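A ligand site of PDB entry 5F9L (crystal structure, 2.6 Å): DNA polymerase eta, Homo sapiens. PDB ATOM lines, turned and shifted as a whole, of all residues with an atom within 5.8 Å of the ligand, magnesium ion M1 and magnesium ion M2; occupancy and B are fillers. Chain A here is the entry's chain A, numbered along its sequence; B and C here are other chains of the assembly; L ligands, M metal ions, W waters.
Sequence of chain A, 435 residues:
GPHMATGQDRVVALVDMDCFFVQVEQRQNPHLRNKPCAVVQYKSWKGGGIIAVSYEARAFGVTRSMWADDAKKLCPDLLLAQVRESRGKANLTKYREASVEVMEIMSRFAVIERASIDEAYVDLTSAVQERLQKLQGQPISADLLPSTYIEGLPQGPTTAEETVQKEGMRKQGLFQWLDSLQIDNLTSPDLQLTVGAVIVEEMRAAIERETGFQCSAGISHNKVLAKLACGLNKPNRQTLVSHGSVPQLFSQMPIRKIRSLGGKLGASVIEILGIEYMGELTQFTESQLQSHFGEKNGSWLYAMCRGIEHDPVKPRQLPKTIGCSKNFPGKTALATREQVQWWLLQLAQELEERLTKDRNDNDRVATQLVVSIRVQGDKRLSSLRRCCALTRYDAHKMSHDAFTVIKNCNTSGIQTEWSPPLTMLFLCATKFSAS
Residues that only touch magnesium ion M2: DT 8 of chain C (2.9 Å).
Of the 25 residues printed, 4 come within 4 Å of magnesium ion M2.
Within 4 Å of magnesium ion M1: Asp 16, Met 17 and Asp 118.
Magnesium ion M1 is bound by O5 of the ligand (2.0 Å), OD2 of Asp 16 (2.2 Å), O9 of the ligand (2.2 Å), OD2 of Asp 118 (2.3 Å), O4 of the ligand (2.3 Å) and O of Met 17 (2.3 Å).
Water W3 bridges an oxygen (O3) of the ligand (2.5 Å) and the guanidinium group of Arg 64 (3.2 Å).
Water W2 bridges an oxygen (O1) of the ligand (2.9 Å) and the guanidinium group (NH2) of Arg 64 (3.4 Å).
Water W5 lies within hydrogen-bond range of OE1 of Gln 41 (2.6 Å) and O4' of DA 5 of chain B (3.2 Å).
The side-chain hydroxyl (OH) of Tyr 55 lies close to the guanidinium group (NH1) of Arg 58, 3.3 Å away.
The side-chain carboxylate (OD1) of Asp 118 sits at hydrogen-bond distance from the side-chain hydroxyl (OG) of Ser 116, at 2.7 Å.
NZ of Lys 234 lies within salt-bridge range of OD1 of Asp 18 (2.5 Å).
OP1 of DT 8 of chain C is in salt-bridge range of NZ of Lys 227 (3.0 Å).
N1 of DA 5 of chain B sits close to N3 of DT 8 of chain C.
The backbone carbonyl oxygen (O) of Asp 16 is in hydrogen-bond range of the side-chain amino group (NZ) of Lys 234, at 3.4 Å.
The side-chain hydroxyl (OG) of Ser 116 sits close to the backbone NH (N) of Glu 119 (3.5 Å).
O3' of DT 8 of chain C lies within hydrogen-bond range of the side-chain hydroxyl of Ser 116.
O4 of the ligand sits close to O3' of DT 8 of chain C (3.4 Å).
CA of Asp 18 touches O6 of the ligand (3.5 Å).
O of Ile 51 touches C7 of the ligand (3.3 Å).
Ala 52 touches the ligand (CB to O7, 3.6 Å).
Ile 117 touches the ligand.
The guanidinium group of Arg 58 lies within salt-bridge range of an oxygen (O3) of the ligand, 3.1 Å away.
The backbone NH (N) of Cys 19 sits at hydrogen-bond distance from an oxygen (O8) of the ligand.
The side-chain amino group (NZ) of Lys 234 lies within salt-bridge range of an oxygen (O6) of the ligand, 3.2 Å away.
The backbone NH (N) of Phe 20 sits at hydrogen-bond distance from an oxygen (O7) of the ligand, 3.3 Å away.
The backbone NH (N) of Phe 21 lies within hydrogen-bond range of an oxygen (O7) of the ligand, at 2.9 Å.
An oxygen (O1) of the ligand lies within salt-bridge range of the guanidinium group (NH1) of Arg 64.
A nitrogen (N3) of the ligand is in hydrogen-bond range of O6 of GNE 4 of chain B (2.9 Å).
OH of Tyr 55 lies within hydrogen-bond range of O6 of the ligand (2.4 Å).
O4 of DT 3 of chain B lies within hydrogen-bond range of a nitrogen (N3) of the ligand, 2.5 Å away.
Magnesium ion M2 is bound by OE2 of Glu 119, O4 of the ligand and OD1 of Asp 16.
Slightly farther from magnesium ion M2 lies the side-chain carboxylate (OD1) of Asp 118 (2.7 Å).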
ATOM      1  N   ASP A  16      10.560 -31.643 -10.061  1.00  0.00           N
ATOM      2  CA  ASP A  16      10.816 -30.421  -9.306  1.00  0.00           C
ATOM      3  C   ASP A  16      11.064 -29.272 -10.271  1.00  0.00           C
ATOM      4  O   ASP A  16      11.876 -29.395 -11.185  1.00  0.00           O
ATOM      5  CB  ASP A  16      12.017 -30.594  -8.374  1.00  0.00           C
ATOM      6  CG  ASP A  16      12.247 -29.381  -7.488  1.00  0.00           C
ATOM      7  OD1 ASP A  16      11.805 -29.409  -6.318  1.00  0.00           O
ATOM      8  OD2 ASP A  16      12.856 -28.406  -7.968  1.00  0.00           O
ATOM      9  N   MET A  17      10.360 -28.161 -10.067  1.00  0.00           N
ATOM     10  CA  MET A  17      10.484 -27.022 -10.957  1.00  0.00           C
ATOM     11  C   MET A  17      11.822 -26.312 -10.753  1.00  0.00           C
ATOM     12  O   MET A  17      12.246 -26.087  -9.611  1.00  0.00           O
ATOM     13  CB  MET A  17       9.336 -26.036 -10.733  1.00  0.00           C
ATOM     14  CG  MET A  17       7.945 -26.656 -10.719  1.00  0.00           C
ATOM     15  SD  MET A  17       7.599 -27.695 -12.150  1.00  0.00           S
ATOM     16  CE  MET A  17       7.877 -26.527 -13.476  1.00  0.00           C
ATOM     17  N   ASP A  18      12.476 -25.964 -11.859  1.00  0.00           N
ATOM     18  CA  ASP A  18      13.760 -25.283 -11.805  1.00  0.00           C
ATOM     19  C   ASP A  18      13.553 -23.814 -11.466  1.00  0.00           C
ATOM     20  O   ASP A  18      12.818 -23.109 -12.180  1.00  0.00           O
ATOM     21  CB  ASP A  18      14.487 -25.423 -13.148  1.00  0.00           C
ATOM     22  CG  ASP A  18      14.767 -26.863 -13.508  1.00  0.00           C
ATOM     23  OD1 ASP A  18      14.923 -27.695 -12.588  1.00  0.00           O
ATOM     24  OD2 ASP A  18      14.835 -27.176 -14.716  1.00  0.00           O
ATOM     25  N   CYS A  19      14.215 -23.343 -10.407  1.00  0.00           N
ATOM     26  CA  CYS A  19      14.065 -21.987  -9.867  1.00  0.00           C
ATOM     27  C   CYS A  19      12.647 -21.465 -10.045  1.00  0.00           C
ATOM     28  O   CYS A  19      12.410 -20.526 -10.804  1.00  0.00           O
ATOM     29  CB  CYS A  19      15.086 -21.036 -10.506  1.00  0.00           C
ATOM     30  SG  CYS A  19      15.185 -21.030 -12.315  1.00  0.00           S
ATOM     31  N   PHE A  20      11.698 -22.095  -9.337  1.00  0.00           N
ATOM     32  CA  PHE A  20      10.286 -21.963  -9.692  1.00  0.00           C
ATOM     33  C   PHE A  20       9.809 -20.522  -9.585  1.00  0.00           C
ATOM     34  O   PHE A  20       9.198 -19.988 -10.527  1.00  0.00           O
ATOM     35  CB  PHE A  20       9.446 -22.876  -8.818  1.00  0.00           C
ATOM     36  CG  PHE A  20       7.982 -22.862  -9.158  1.00  0.00           C
ATOM     37  CD1 PHE A  20       7.571 -23.013 -10.476  1.00  0.00           C
ATOM     38  CD2 PHE A  20       7.034 -22.689  -8.175  1.00  0.00           C
ATOM     39  CE1 PHE A  20       6.225 -23.000 -10.792  1.00  0.00           C
ATOM     40  CE2 PHE A  20       5.688 -22.675  -8.491  1.00  0.00           C
ATOM     41  CZ  PHE A  20       5.286 -22.824  -9.799  1.00  0.00           C
ATOM     42  N   PHE A  21      10.061 -19.869  -8.447  1.00  0.00           N
ATOM     43  CA  PHE A  21       9.598 -18.493  -8.275  1.00  0.00           C
ATOM     44  C   PHE A  21      10.200 -17.578  -9.340  1.00  0.00           C
ATOM     45  O   PHE A  21       9.534 -16.652  -9.822  1.00  0.00           O
ATOM     46  CB  PHE A  21       9.942 -17.987  -6.880  1.00  0.00           C
ATOM     47  CG  PHE A  21       9.051 -18.530  -5.787  1.00  0.00           C
ATOM     48  CD1 PHE A  21       8.323 -19.698  -5.978  1.00  0.00           C
ATOM     49  CD2 PHE A  21       8.938 -17.870  -4.574  1.00  0.00           C
ATOM     50  CE1 PHE A  21       7.514 -20.204  -4.966  1.00  0.00           C
ATOM     51  CE2 PHE A  21       8.125 -18.366  -3.572  1.00  0.00           C
ATOM     52  CZ  PHE A  21       7.419 -19.536  -3.773  1.00  0.00           C
ATOM     53  N   VAL A  22      11.452 -17.826  -9.719  1.00  0.00           N
ATOM     54  CA  VAL A  22      12.088 -17.030 -10.764  1.00  0.00           C
ATOM     55  C   VAL A  22      11.390 -17.244 -12.104  1.00  0.00           C
ATOM     56  O   VAL A  22      11.085 -16.292 -12.820  1.00  0.00           O
ATOM     57  CB  VAL A  22      13.590 -17.360 -10.837  1.00  0.00           C
ATOM     58  CG1 VAL A  22      14.173 -16.891 -12.163  1.00  0.00           C
ATOM     59  CG2 VAL A  22      14.333 -16.705  -9.679  1.00  0.00           C
ATOM     60  N   GLN A  41      11.941 -10.854  -0.798  1.00  0.00           N
ATOM     61  CA  GLN A  41      10.893 -10.334   0.072  1.00  0.00           C
ATOM     62  C   GLN A  41      11.439  -9.144   0.843  1.00  0.00           C
ATOM     63  O   GLN A  41      12.571  -9.178   1.337  1.00  0.00           O
ATOM     64  CB  GLN A  41      10.382 -11.380   1.065  1.00  0.00           C
ATOM     65  CG  GLN A  41      10.173 -12.774   0.517  1.00  0.00           C
ATOM     66  CD  GLN A  41       9.912 -13.798   1.612  1.00  0.00           C
ATOM     67  OE1 GLN A  41       9.320 -14.846   1.364  1.00  0.00           O
ATOM     68  NE2 GLN A  41      10.358 -13.486   2.829  1.00  0.00           N
ATOM     69  N   ILE A  51      14.961 -15.573  -2.044  1.00  0.00           N
ATOM     70  CA  ILE A  51      14.278 -16.844  -1.832  1.00  0.00           C
ATOM     71  C   ILE A  51      14.285 -17.735  -3.067  1.00  0.00           C
ATOM     72  O   ILE A  51      13.816 -18.870  -2.994  1.00  0.00           O
ATOM     73  CB  ILE A  51      12.838 -16.633  -1.338  1.00  0.00           C
ATOM     74  CG1 ILE A  51      11.977 -16.008  -2.434  1.00  0.00           C
ATOM     75  CG2 ILE A  51      12.826 -15.756  -0.084  1.00  0.00           C
ATOM     76  CD1 ILE A  51      10.531 -15.813  -2.021  1.00  0.00           C
ATOM     77  N   ALA A  52      14.813 -17.250  -4.189  1.00  0.00           N
ATOM     78  CA  ALA A  52      14.906 -18.057  -5.401  1.00  0.00           C
ATOM     79  C   ALA A  52      15.915 -17.397  -6.340  1.00  0.00           C
ATOM     80  O   ALA A  52      15.889 -16.171  -6.506  1.00  0.00           O
ATOM     81  CB  ALA A  52      13.549 -18.198  -6.098  1.00  0.00           C
ATOM     82  N   VAL A  53      16.786 -18.200  -6.921  1.00  0.00           N
ATOM     83  CA  VAL A  53      17.895 -17.715  -7.746  1.00  0.00           C
ATOM     84  C   VAL A  53      17.836 -18.406  -9.105  1.00  0.00           C
ATOM     85  O   VAL A  53      17.697 -19.631  -9.172  1.00  0.00           O
ATOM     86  CB  VAL A  53      19.251 -17.969  -7.076  1.00  0.00           C
ATOM     87  CG1 VAL A  53      20.340 -17.170  -7.768  1.00  0.00           C
ATOM     88  CG2 VAL A  53      19.202 -17.639  -5.597  1.00  0.00           C
ATOM     89  N   TYR A  55      19.617 -19.728 -12.607  1.00  0.00           N
ATOM     90  CA  TYR A  55      20.897 -20.410 -12.796  1.00  0.00           C
ATOM     91  C   TYR A  55      21.959 -19.480 -13.388  1.00  0.00           C
ATOM     92  O   TYR A  55      23.151 -19.684 -13.149  1.00  0.00           O
ATOM     93  CB  TYR A  55      20.710 -21.651 -13.665  1.00  0.00           C
ATOM     94  CG  TYR A  55      20.123 -22.814 -12.898  1.00  0.00           C
ATOM     95  CD1 TYR A  55      18.764 -22.855 -12.605  1.00  0.00           C
ATOM     96  CD2 TYR A  55      20.928 -23.855 -12.460  1.00  0.00           C
ATOM     97  CE1 TYR A  55      18.222 -23.911 -11.892  1.00  0.00           C
ATOM     98  CE2 TYR A  55      20.389 -24.920 -11.748  1.00  0.00           C
ATOM     99  CZ  TYR A  55      19.045 -24.945 -11.464  1.00  0.00           C
ATOM    100  OH  TYR A  55      18.502 -26.000 -10.762  1.00  0.00           O
ATOM    101  N   ARG A  58      23.210 -18.025 -10.300  1.00  0.00           N
ATOM    102  CA  ARG A  58      23.947 -18.984  -9.482  1.00  0.00           C
ATOM    103  C   ARG A  58      25.395 -19.130  -9.952  1.00  0.00           C
ATOM    104  O   ARG A  58      26.265 -19.480  -9.159  1.00  0.00           O
ATOM    105  CB  ARG A  58      23.252 -20.347  -9.497  1.00  0.00           C
ATOM    106  CG  ARG A  58      21.851 -20.321  -8.916  1.00  0.00           C
ATOM    107  CD  ARG A  58      21.204 -21.698  -8.944  1.00  0.00           C
ATOM    108  NE  ARG A  58      19.768 -21.622  -8.740  1.00  0.00           N
ATOM    109  CZ  ARG A  58      18.979 -22.667  -8.498  1.00  0.00           C
ATOM    110  NH1 ARG A  58      19.493 -23.884  -8.411  1.00  0.00           N
ATOM    111  NH2 ARG A  58      17.674 -22.485  -8.332  1.00  0.00           N
ATOM    112  N   ARG A  64      20.337 -18.647  -2.271  1.00  0.00           N
ATOM    113  CA  ARG A  64      19.182 -18.357  -1.442  1.00  0.00           C
ATOM    114  C   ARG A  64      19.632 -18.049  -0.015  1.00  0.00           C
ATOM    115  O   ARG A  64      20.742 -18.396   0.398  1.00  0.00           O
ATOM    116  CB  ARG A  64      18.191 -19.529  -1.481  1.00  0.00           C
ATOM    117  CG  ARG A  64      17.099 -19.512  -0.433  1.00  0.00           C
ATOM    118  CD  ARG A  64      16.301 -20.797  -0.438  1.00  0.00           C
ATOM    119  NE  ARG A  64      17.146 -21.945  -0.731  1.00  0.00           N
ATOM    120  CZ  ARG A  64      16.837 -22.863  -1.643  1.00  0.00           C
ATOM    121  NH1 ARG A  64      15.711 -22.768  -2.333  1.00  0.00           N
ATOM    122  NH2 ARG A  64      17.667 -23.884  -1.857  1.00  0.00           N
ATOM    123  N   SER A 116       5.959 -30.266  -2.177  1.00  0.00           N
ATOM    124  CA  SER A 116       6.155 -28.871  -1.839  1.00  0.00           C
ATOM    125  C   SER A 116       5.365 -28.034  -2.844  1.00  0.00           C
ATOM    126  O   SER A 116       4.568 -28.558  -3.619  1.00  0.00           O
ATOM    127  CB  SER A 116       7.642 -28.507  -1.825  1.00  0.00           C
ATOM    128  OG  SER A 116       8.074 -28.057  -3.096  1.00  0.00           O
ATOM    129  N   ILE A 117       5.609 -26.723  -2.824  1.00  0.00           N
ATOM    130  CA  ILE A 117       4.911 -25.845  -3.770  1.00  0.00           C
ATOM    131  C   ILE A 117       5.401 -26.067  -5.199  1.00  0.00           C
ATOM    132  O   ILE A 117       4.678 -25.745  -6.151  1.00  0.00           O
ATOM    133  CB  ILE A 117       5.079 -24.371  -3.345  1.00  0.00           C
ATOM    134  CG1 ILE A 117       4.099 -23.476  -4.107  1.00  0.00           C
ATOM    135  CG2 ILE A 117       6.503 -23.905  -3.552  1.00  0.00           C
ATOM    136  CD1 ILE A 117       4.117 -22.028  -3.658  1.00  0.00           C
ATOM    137  N   ASP A 118       6.595 -26.633  -5.376  1.00  0.00           N
ATOM    138  CA  ASP A 118       7.195 -26.747  -6.702  1.00  0.00           C
ATOM    139  C   ASP A 118       7.561 -28.187  -7.066  1.00  0.00           C
ATOM    140  O   ASP A 118       8.224 -28.399  -8.090  1.00  0.00           O
ATOM    141  CB  ASP A 118       8.450 -25.883  -6.795  1.00  0.00           C
ATOM    142  CG  ASP A 118       9.665 -26.559  -6.188  1.00  0.00           C
ATOM    143  OD1 ASP A 118       9.649 -26.838  -4.972  1.00  0.00           O
ATOM    144  OD2 ASP A 118      10.625 -26.811  -6.936  1.00  0.00           O
ATOM    145  N   GLU A 119       7.164 -29.173  -6.274  1.00  0.00           N
ATOM    146  CA  GLU A 119       7.546 -30.538  -6.563  1.00  0.00           C
ATOM    147  C   GLU A 119       6.471 -31.495  -6.083  1.00  0.00           C
ATOM    148  O   GLU A 119       5.766 -31.232  -5.094  1.00  0.00           O
ATOM    149  CB  GLU A 119       8.898 -30.897  -5.930  1.00  0.00           C
ATOM    150  CG  GLU A 119       8.915 -30.769  -4.428  1.00  0.00           C
ATOM    151  CD  GLU A 119      10.305 -30.550  -3.887  1.00  0.00           C
ATOM    152  OE1 GLU A 119      11.080 -31.529  -3.815  1.00  0.00           O
ATOM    153  OE2 GLU A 119      10.633 -29.394  -3.541  1.00  0.00           O
ATOM    154  N   LYS A 227      14.129 -38.530  -5.579  1.00  0.00           N
ATOM    155  CA  LYS A 227      14.508 -37.166  -5.200  1.00  0.00           C
ATOM    156  C   LYS A 227      16.012 -36.964  -5.348  1.00  0.00           C
ATOM    157  O   LYS A 227      16.456 -35.891  -5.804  1.00  0.00           O
ATOM    158  CB  LYS A 227      14.066 -36.871  -3.778  1.00  0.00           C
ATOM    159  CG  LYS A 227      14.421 -35.469  -3.326  1.00  0.00           C
ATOM    160  CD  LYS A 227      14.042 -35.228  -1.879  1.00  0.00           C
ATOM    161  CE  LYS A 227      14.462 -33.830  -1.460  1.00  0.00           C
ATOM    162  NZ  LYS A 227      13.964 -32.801  -2.423  1.00  0.00           N
ATOM    163  N   LYS A 234      20.292 -31.118 -12.768  1.00  0.00           N
ATOM    164  CA  LYS A 234      19.562 -29.866 -12.944  1.00  0.00           C
ATOM    165  C   LYS A 234      20.441 -28.912 -13.757  1.00  0.00           C
ATOM    166  O   LYS A 234      21.666 -28.983 -13.681  1.00  0.00           O
ATOM    167  CB  LYS A 234      19.190 -29.250 -11.603  1.00  0.00           C
ATOM    168  CG  LYS A 234      17.894 -29.787 -10.995  1.00  0.00           C
ATOM    169  CD  LYS A 234      17.485 -28.993  -9.761  1.00  0.00           C
ATOM    170  CE  LYS A 234      16.032 -29.261  -9.369  1.00  0.00           C
ATOM    171  NZ  LYS A 234      15.058 -28.586 -10.286  1.00  0.00           N
ATOM    172  N   PRO A 235      19.825 -28.017 -14.544  1.00  0.00           N
ATOM    173  CA  PRO A 235      18.382 -27.856 -14.745  1.00  0.00           C
ATOM    174  C   PRO A 235      17.837 -28.501 -16.021  1.00  0.00           C
ATOM    175  O   PRO A 235      18.597 -28.826 -16.927  1.00  0.00           O
ATOM    176  CB  PRO A 235      18.234 -26.330 -14.826  1.00  0.00           C
ATOM    177  CG  PRO A 235      19.496 -25.906 -15.520  1.00  0.00           C
ATOM    178  CD  PRO A 235      20.579 -26.892 -15.130  1.00  0.00           C
ATOM    179  P    DT B   3      20.242 -14.106   9.287  1.00  0.00           P
ATOM    180  OP1  DT B   3      21.294 -14.162  10.324  1.00  0.00           O
ATOM    181  OP2  DT B   3      20.636 -14.300   7.864  1.00  0.00           O
ATOM    182  O5'  DT B   3      19.079 -15.144   9.695  1.00  0.00           O
ATOM    183  C5'  DT B   3      18.373 -15.893   8.690  1.00  0.00           C
ATOM    184  C4'  DT B   3      17.661 -14.976   7.718  1.00  0.00           C
ATOM    185  O4'  DT B   3      17.854 -15.457   6.383  1.00  0.00           O
ATOM    186  C3'  DT B   3      16.143 -14.884   7.876  1.00  0.00           C
ATOM    187  O3'  DT B   3      15.830 -13.872   8.840  1.00  0.00           O
ATOM    188  C2'  DT B   3      15.694 -14.486   6.467  1.00  0.00           C
ATOM    189  C1'  DT B   3      16.807 -15.009   5.553  1.00  0.00           C
ATOM    190  N1   DT B   3      16.372 -16.129   4.682  1.00  0.00           N
ATOM    191  C2   DT B   3      15.644 -15.858   3.546  1.00  0.00           C
ATOM    192  O2   DT B   3      15.330 -14.726   3.205  1.00  0.00           O
ATOM    193  N3   DT B   3      15.301 -16.964   2.803  1.00  0.00           N
ATOM    194  C4   DT B   3      15.607 -18.276   3.092  1.00  0.00           C
ATOM    195  O4   DT B   3      15.252 -19.206   2.361  1.00  0.00           O
ATOM    196  C5   DT B   3      16.362 -18.501   4.300  1.00  0.00           C
ATOM    197  C7   DT B   3      16.752 -19.889   4.712  1.00  0.00           C
ATOM    198  C6   DT B   3      16.705 -17.426   5.032  1.00  0.00           C
ATOM    199  P   GNE B   4      14.326 -13.658   9.407  1.00  0.00           P
ATOM    200  OP1 GNE B   4      14.124 -12.178   9.636  1.00  0.00           O
ATOM    201  OP2 GNE B   4      14.075 -14.447  10.668  1.00  0.00           O
ATOM    202  O5' GNE B   4      13.334 -14.136   8.231  1.00  0.00           O
ATOM    203  C5' GNE B   4      12.682 -13.146   7.422  1.00  0.00           C
ATOM    204  C4' GNE B   4      11.665 -13.804   6.496  1.00  0.00           C
ATOM    205  O4' GNE B   4      12.208 -14.960   5.843  1.00  0.00           O
ATOM    206  C3' GNE B   4      10.416 -14.260   7.238  1.00  0.00           C
ATOM    207  O3' GNE B   4       9.320 -13.526   6.740  1.00  0.00           O
ATOM    208  C2' GNE B   4      10.267 -15.722   6.884  1.00  0.00           C
ATOM    209  C1' GNE B   4      11.100 -15.829   5.619  1.00  0.00           C
ATOM    210  N9  GNE B   4      11.477 -17.237   5.317  1.00  0.00           N
ATOM    211  C8  GNE B   4      10.955 -17.937   4.287  1.00  0.00           C
ATOM    212  N7  GNE B   4      11.468 -19.186   4.232  1.00  0.00           N
ATOM    213  C5  GNE B   4      12.340 -19.307   5.241  1.00  0.00           C
ATOM    214  C6  GNE B   4      13.225 -20.387   5.734  1.00  0.00           C
ATOM    215  O6  GNE B   4      13.259 -21.494   5.156  1.00  0.00           O
ATOM    216  N1  GNE B   4      13.994 -20.144   6.803  1.00  0.00           N
ATOM    217  C2  GNE B   4      13.958 -18.946   7.437  1.00  0.00           C
ATOM    218  N2  GNE B   4      14.829 -19.005   8.461  1.00  0.00           N
ATOM    219  CM2 GNE B   4      15.397 -20.229   8.485  1.00  0.00           C
ATOM    220  N3  GNE B   4      13.167 -17.913   7.028  1.00  0.00           N
ATOM    221  C11 GNE B   4      14.856 -20.934   7.436  1.00  0.00           C
ATOM    222  C4  GNE B   4      12.349 -18.024   5.960  1.00  0.00           C
ATOM    223  P    DA B   5       7.841 -13.777   7.325  1.00  0.00           P
ATOM    224  OP1  DA B   5       7.053 -12.544   7.110  1.00  0.00           O
ATOM    225  OP2  DA B   5       8.003 -14.323   8.696  1.00  0.00           O
ATOM    226  O5'  DA B   5       7.251 -14.940   6.417  1.00  0.00           O
ATOM    227  C5'  DA B   5       7.349 -14.860   4.994  1.00  0.00           C
ATOM    228  C4'  DA B   5       6.768 -16.096   4.352  1.00  0.00           C
ATOM    229  O4'  DA B   5       7.726 -17.189   4.419  1.00  0.00           O
ATOM    230  C3'  DA B   5       5.490 -16.621   5.020  1.00  0.00           C
ATOM    231  O3'  DA B   5       4.565 -17.068   4.034  1.00  0.00           O
ATOM    232  C2'  DA B   5       6.008 -17.762   5.874  1.00  0.00           C
ATOM    233  C1'  DA B   5       7.101 -18.317   4.990  1.00  0.00           C
ATOM    234  N9   DA B   5       8.101 -19.096   5.729  1.00  0.00           N
ATOM    235  C8   DA B   5       8.584 -18.826   6.981  1.00  0.00           C
ATOM    236  N7   DA B   5       9.467 -19.708   7.397  1.00  0.00           N
ATOM    237  C5   DA B   5       9.559 -20.615   6.359  1.00  0.00           C
ATOM    238  C6   DA B   5      10.317 -21.784   6.188  1.00  0.00           C
ATOM    239  N6   DA B   5      11.172 -22.258   7.104  1.00  0.00           N
ATOM    240  N1   DA B   5      10.170 -22.461   5.025  1.00  0.00           N
ATOM    241  C2   DA B   5       9.315 -21.987   4.108  1.00  0.00           C
ATOM    242  N3   DA B   5       8.546 -20.909   4.163  1.00  0.00           N
ATOM    243  C4   DA B   5       8.714 -20.257   5.324  1.00  0.00           C
ATOM    244  P    DT C   8      14.645 -30.057   0.755  1.00  0.00           P
ATOM    245  OP1  DT C   8      15.082 -30.868  -0.401  1.00  0.00           O
ATOM    246  OP2  DT C   8      15.657 -29.336   1.555  1.00  0.00           O
ATOM    247  O5'  DT C   8      13.564 -28.995   0.249  1.00  0.00           O
ATOM    248  C5'  DT C   8      12.323 -29.439  -0.282  1.00  0.00           C
ATOM    249  C4'  DT C   8      11.379 -28.274  -0.506  1.00  0.00           C
ATOM    250  O4'  DT C   8      11.107 -27.615   0.764  1.00  0.00           O
ATOM    251  C3'  DT C   8      11.906 -27.185  -1.436  1.00  0.00           C
ATOM    252  O3'  DT C   8      10.876 -26.728  -2.306  1.00  0.00           O
ATOM    253  C2'  DT C   8      12.361 -26.087  -0.477  1.00  0.00           C
ATOM    254  C1'  DT C   8      11.355 -26.237   0.647  1.00  0.00           C
ATOM    255  N1   DT C   8      11.857 -25.729   1.955  1.00  0.00           N
ATOM    256  C2   DT C   8      11.092 -24.832   2.669  1.00  0.00           C
ATOM    257  O2   DT C   8      10.013 -24.424   2.289  1.00  0.00           O
ATOM    258  N3   DT C   8      11.634 -24.438   3.858  1.00  0.00           N
ATOM    259  C4   DT C   8      12.848 -24.831   4.394  1.00  0.00           C
ATOM    260  O4   DT C   8      13.253 -24.416   5.479  1.00  0.00           O
ATOM    261  C5   DT C   8      13.605 -25.766   3.597  1.00  0.00           C
ATOM    262  C7   DT C   8      14.936 -26.271   4.080  1.00  0.00           C
ATOM    263  C6   DT C   8      13.076 -26.167   2.428  1.00  0.00           C
HETATM  264  N1  LIG L   1      12.390 -19.465   1.698  1.00  0.00           N
HETATM  265  C1  LIG L   1      11.485 -18.911   0.879  1.00  0.00           C
HETATM  266  N2  LIG L   1      11.047 -19.496  -0.246  1.00  0.00           N
HETATM  267  C2  LIG L   1      11.522 -20.713  -0.609  1.00  0.00           C
HETATM  268  C3  LIG L   1      12.514 -21.385   0.238  1.00  0.00           C
HETATM  269  C4  LIG L   1      12.929 -20.678   1.463  1.00  0.00           C
HETATM  270  N3  LIG L   1      13.841 -21.221   2.312  1.00  0.00           N
HETATM  271  N4  LIG L   1      12.798 -22.558  -0.355  1.00  0.00           N
HETATM  272  C5  LIG L   1      12.058 -22.624  -1.483  1.00  0.00           C
HETATM  273  N5  LIG L   1      11.290 -21.528  -1.638  1.00  0.00           N
HETATM  274  P1  LIG L   1      13.530 -25.204  -4.397  1.00  0.00           P
HETATM  275  P2  LIG L   1      14.306 -23.811  -6.821  1.00  0.00           P
HETATM  276  P3  LIG L   1      16.010 -25.549  -8.112  1.00  0.00           P
HETATM  277  C6  LIG L   1      10.369 -21.256  -2.756  1.00  0.00           C
HETATM  278  O1  LIG L   1      14.151 -25.719  -3.002  1.00  0.00           O
HETATM  279  O2  LIG L   1      14.198 -22.237  -6.519  1.00  0.00           O
HETATM  280  O3  LIG L   1      17.226 -25.649  -7.215  1.00  0.00           O
HETATM  281  C7  LIG L   1      11.132 -20.515  -3.840  1.00  0.00           C
HETATM  282  O4  LIG L   1      12.826 -26.311  -5.076  1.00  0.00           O
HETATM  283  O5  LIG L   1      12.973 -24.319  -7.243  1.00  0.00           O
HETATM  284  O6  LIG L   1      16.407 -25.783  -9.559  1.00  0.00           O
HETATM  285  C8  LIG L   1      11.483 -21.573  -4.859  1.00  0.00           C
HETATM  286  O7  LIG L   1      11.346 -21.064  -6.183  1.00  0.00           O
HETATM  287  N6  LIG L   1      14.881 -24.657  -5.387  1.00  0.00           N
HETATM  288  O8  LIG L   1      15.393 -24.078  -7.977  1.00  0.00           O
HETATM  289  O9  LIG L   1      14.960 -26.547  -7.686  1.00  0.00           O
HETATM  290  C9  LIG L   1      10.492 -22.706  -4.605  1.00  0.00           C
HETATM  291  O10 LIG L   1       9.944 -22.505  -3.305  1.00  0.00           O
HETATM  292  C10 LIG L   1      11.186 -24.068  -4.666  1.00  0.00           C
HETATM  293  O11 LIG L   1      12.501 -23.993  -4.142  1.00  0.00           O
HETATM  294 MG    MG M   1      12.802 -26.311  -7.372  1.00  0.00          MG
HETATM  295 MG    MG M   2      11.908 -28.166  -4.573  1.00  0.00          MG
HETATM  296  O   HOH W   1      15.345 -28.241  -5.289  1.00  0.00           O
HETATM  297  O   HOH W   2      16.626 -27.100  -2.404  1.00  0.00           O
HETATM  298  O   HOH W   3      17.492 -24.985  -4.854  1.00  0.00           O
HETATM  299  O   HOH W   4      15.689 -23.330   2.775  1.00  0.00           O
HETATM  300  O   HOH W   5       8.701 -17.402   1.346  1.00  0.00           O
